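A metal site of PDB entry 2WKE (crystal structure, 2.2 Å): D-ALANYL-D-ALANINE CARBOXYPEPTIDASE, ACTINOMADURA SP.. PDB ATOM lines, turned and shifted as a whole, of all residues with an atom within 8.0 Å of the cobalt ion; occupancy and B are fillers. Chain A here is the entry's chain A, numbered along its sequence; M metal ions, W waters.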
ATOM      1  N   GLY A 185     -22.184  31.022  18.958  1.00  0.00           N
ATOM      2  CA  GLY A 185     -22.188  32.098  19.952  1.00  0.00           C
ATOM      3  C   GLY A 185     -22.974  31.698  21.186  1.00  0.00           C
ATOM      4  O   GLY A 185     -22.858  30.563  21.668  1.00  0.00           O
ATOM      5  N   ALA A 186     -23.764  32.633  21.695  1.00  0.00           N
ATOM      6  CA  ALA A 186     -24.558  32.407  22.895  1.00  0.00           C
ATOM      7  C   ALA A 186     -25.493  31.210  22.727  1.00  0.00           C
ATOM      8  O   ALA A 186     -25.747  30.462  23.676  1.00  0.00           O
ATOM      9  CB  ALA A 186     -25.332  33.660  23.259  1.00  0.00           C
ATOM     10  N   ALA A 187     -25.988  31.034  21.505  1.00  0.00           N
ATOM     11  CA  ALA A 187     -26.953  30.013  21.139  1.00  0.00           C
ATOM     12  C   ALA A 187     -26.355  28.620  20.939  1.00  0.00           C
ATOM     13  O   ALA A 187     -27.095  27.693  20.558  1.00  0.00           O
ATOM     14  CB  ALA A 187     -27.725  30.432  19.878  1.00  0.00           C
ATOM     15  N   GLU A 188     -25.048  28.463  21.141  1.00  0.00           N
ATOM     16  CA  GLU A 188     -24.452  27.130  21.194  1.00  0.00           C
ATOM     17  C   GLU A 188     -25.163  26.382  22.309  1.00  0.00           C
ATOM     18  O   GLU A 188     -25.205  26.847  23.461  1.00  0.00           O
ATOM     19  CB  GLU A 188     -22.956  27.176  21.525  1.00  0.00           C
ATOM     20  CG  GLU A 188     -22.031  27.473  20.352  1.00  0.00           C
ATOM     21  CD  GLU A 188     -21.736  26.254  19.448  1.00  0.00           C
ATOM     22  OE1 GLU A 188     -22.315  25.144  19.670  1.00  0.00           O
ATOM     23  OE2 GLU A 188     -20.909  26.415  18.509  1.00  0.00           O
ATOM     24  N   GLY A 189     -25.762  25.251  21.962  1.00  0.00           N
ATOM     25  CA  GLY A 189     -26.482  24.436  22.919  1.00  0.00           C
ATOM     26  C   GLY A 189     -27.946  24.829  23.047  1.00  0.00           C
ATOM     27  O   GLY A 189     -28.698  24.201  23.783  1.00  0.00           O
ATOM     28  N   TYR A 190     -28.334  25.880  22.325  1.00  0.00           N
ATOM     29  CA  TYR A 190     -29.689  26.356  22.315  1.00  0.00           C
ATOM     30  C   TYR A 190     -30.343  26.222  20.937  1.00  0.00           C
ATOM     31  O   TYR A 190     -31.400  25.611  20.812  1.00  0.00           O
ATOM     32  CB  TYR A 190     -29.788  27.812  22.811  1.00  0.00           C
ATOM     33  CG  TYR A 190     -31.217  28.263  22.753  1.00  0.00           C
ATOM     34  CD1 TYR A 190     -32.176  27.676  23.567  1.00  0.00           C
ATOM     35  CD2 TYR A 190     -31.626  29.215  21.817  1.00  0.00           C
ATOM     36  CE1 TYR A 190     -33.495  28.051  23.480  1.00  0.00           C
ATOM     37  CE2 TYR A 190     -32.948  29.600  21.732  1.00  0.00           C
ATOM     38  CZ  TYR A 190     -33.885  29.017  22.567  1.00  0.00           C
ATOM     39  OH  TYR A 190     -35.206  29.381  22.490  1.00  0.00           O
ATOM     40  N   ALA A 191     -29.731  26.829  19.921  1.00  0.00           N
ATOM     41  CA  ALA A 191     -30.179  26.661  18.533  1.00  0.00           C
ATOM     42  C   ALA A 191     -29.511  25.436  17.912  1.00  0.00           C
ATOM     43  O   ALA A 191     -28.458  25.003  18.378  1.00  0.00           O
ATOM     44  CB  ALA A 191     -29.857  27.891  17.722  1.00  0.00           C
ATOM     45  N   LEU A 244     -33.375  31.469  25.429  1.00  0.00           N
ATOM     46  CA  LEU A 244     -31.934  31.685  25.337  1.00  0.00           C
ATOM     47  C   LEU A 244     -31.421  32.314  26.626  1.00  0.00           C
ATOM     48  O   LEU A 244     -30.405  31.869  27.173  1.00  0.00           O
ATOM     49  CB  LEU A 244     -31.537  32.529  24.103  1.00  0.00           C
ATOM     50  CG  LEU A 244     -30.004  32.659  23.885  1.00  0.00           C
ATOM     51  CD1 LEU A 244     -29.312  31.295  23.733  1.00  0.00           C
ATOM     52  CD2 LEU A 244     -29.657  33.581  22.717  1.00  0.00           C
ATOM     53  N   HIS A 247     -31.254  29.414  29.024  1.00  0.00           N
ATOM     54  CA  HIS A 247     -30.076  28.581  28.720  1.00  0.00           C
ATOM     55  C   HIS A 247     -28.771  29.235  29.176  1.00  0.00           C
ATOM     56  O   HIS A 247     -27.927  28.583  29.791  1.00  0.00           O
ATOM     57  CB  HIS A 247     -30.012  28.260  27.211  1.00  0.00           C
ATOM     58  CG  HIS A 247     -28.741  27.587  26.786  1.00  0.00           C
ATOM     59  ND1 HIS A 247     -28.549  26.220  26.891  1.00  0.00           N
ATOM     60  CD2 HIS A 247     -27.587  28.084  26.260  1.00  0.00           C
ATOM     61  CE1 HIS A 247     -27.344  25.912  26.468  1.00  0.00           C
ATOM     62  NE2 HIS A 247     -26.743  27.014  26.066  1.00  0.00           N
ATOM     63  N   LEU A 248     -28.596  30.512  28.872  1.00  0.00           N
ATOM     64  CA  LEU A 248     -27.410  31.242  29.285  1.00  0.00           C
ATOM     65  C   LEU A 248     -27.302  31.418  30.806  1.00  0.00           C
ATOM     66  O   LEU A 248     -26.205  31.527  31.341  1.00  0.00           O
ATOM     67  CB  LEU A 248     -27.336  32.615  28.592  1.00  0.00           C
ATOM     68  CG  LEU A 248     -27.037  32.626  27.086  1.00  0.00           C
ATOM     69  CD1 LEU A 248     -27.191  34.062  26.553  1.00  0.00           C
ATOM     70  CD2 LEU A 248     -25.656  32.038  26.724  1.00  0.00           C
ATOM     71  N   GLU A 250     -28.536  29.277  33.049  1.00  0.00           N
ATOM     72  CA  GLU A 250     -28.159  27.920  33.442  1.00  0.00           C
ATOM     73  C   GLU A 250     -26.640  27.782  33.389  1.00  0.00           C
ATOM     74  O   GLU A 250     -26.021  27.310  34.338  1.00  0.00           O
ATOM     75  CB  GLU A 250     -28.880  26.939  32.517  1.00  0.00           C
ATOM     76  CG  GLU A 250     -28.143  25.668  32.121  1.00  0.00           C
ATOM     77  CD  GLU A 250     -28.495  24.531  32.999  1.00  0.00           C
ATOM     78  OE1 GLU A 250     -28.151  24.642  34.186  1.00  0.00           O
ATOM     79  OE2 GLU A 250     -29.123  23.552  32.528  1.00  0.00           O
ATOM     80  N   GLU A 251     -26.031  28.259  32.297  1.00  0.00           N
ATOM     81  CA  GLU A 251     -24.578  28.305  32.163  1.00  0.00           C
ATOM     82  C   GLU A 251     -23.879  29.151  33.236  1.00  0.00           C
ATOM     83  O   GLU A 251     -22.900  28.706  33.833  1.00  0.00           O
ATOM     84  CB  GLU A 251     -24.179  28.715  30.742  1.00  0.00           C
ATOM     85  CG  GLU A 251     -24.457  27.605  29.735  1.00  0.00           C
ATOM     86  CD  GLU A 251     -24.353  28.041  28.281  1.00  0.00           C
ATOM     87  OE1 GLU A 251     -24.116  27.155  27.445  1.00  0.00           O
ATOM     88  OE2 GLU A 251     -24.520  29.249  27.963  1.00  0.00           O
HETATM   89 CO    CO M   1     -24.729  26.993  25.515  1.00  0.00          CO
HETATM   90  O   HOH W   1     -24.348  29.266  25.377  1.00  0.00           O
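The cobalt ion is bound by the side-chain carboxylate (OE1) of Glu 251, a ring nitrogen (NE2) of His 247, the backbone carbonyl oxygen (O) of Glu 188 and water W1. The cobalt ion has four donor atoms within binding distance.
Water W1 lies within hydrogen-bond range of O of Ala 186 (2.5 Å) and OE2 of Glu 251 (2.6 Å).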
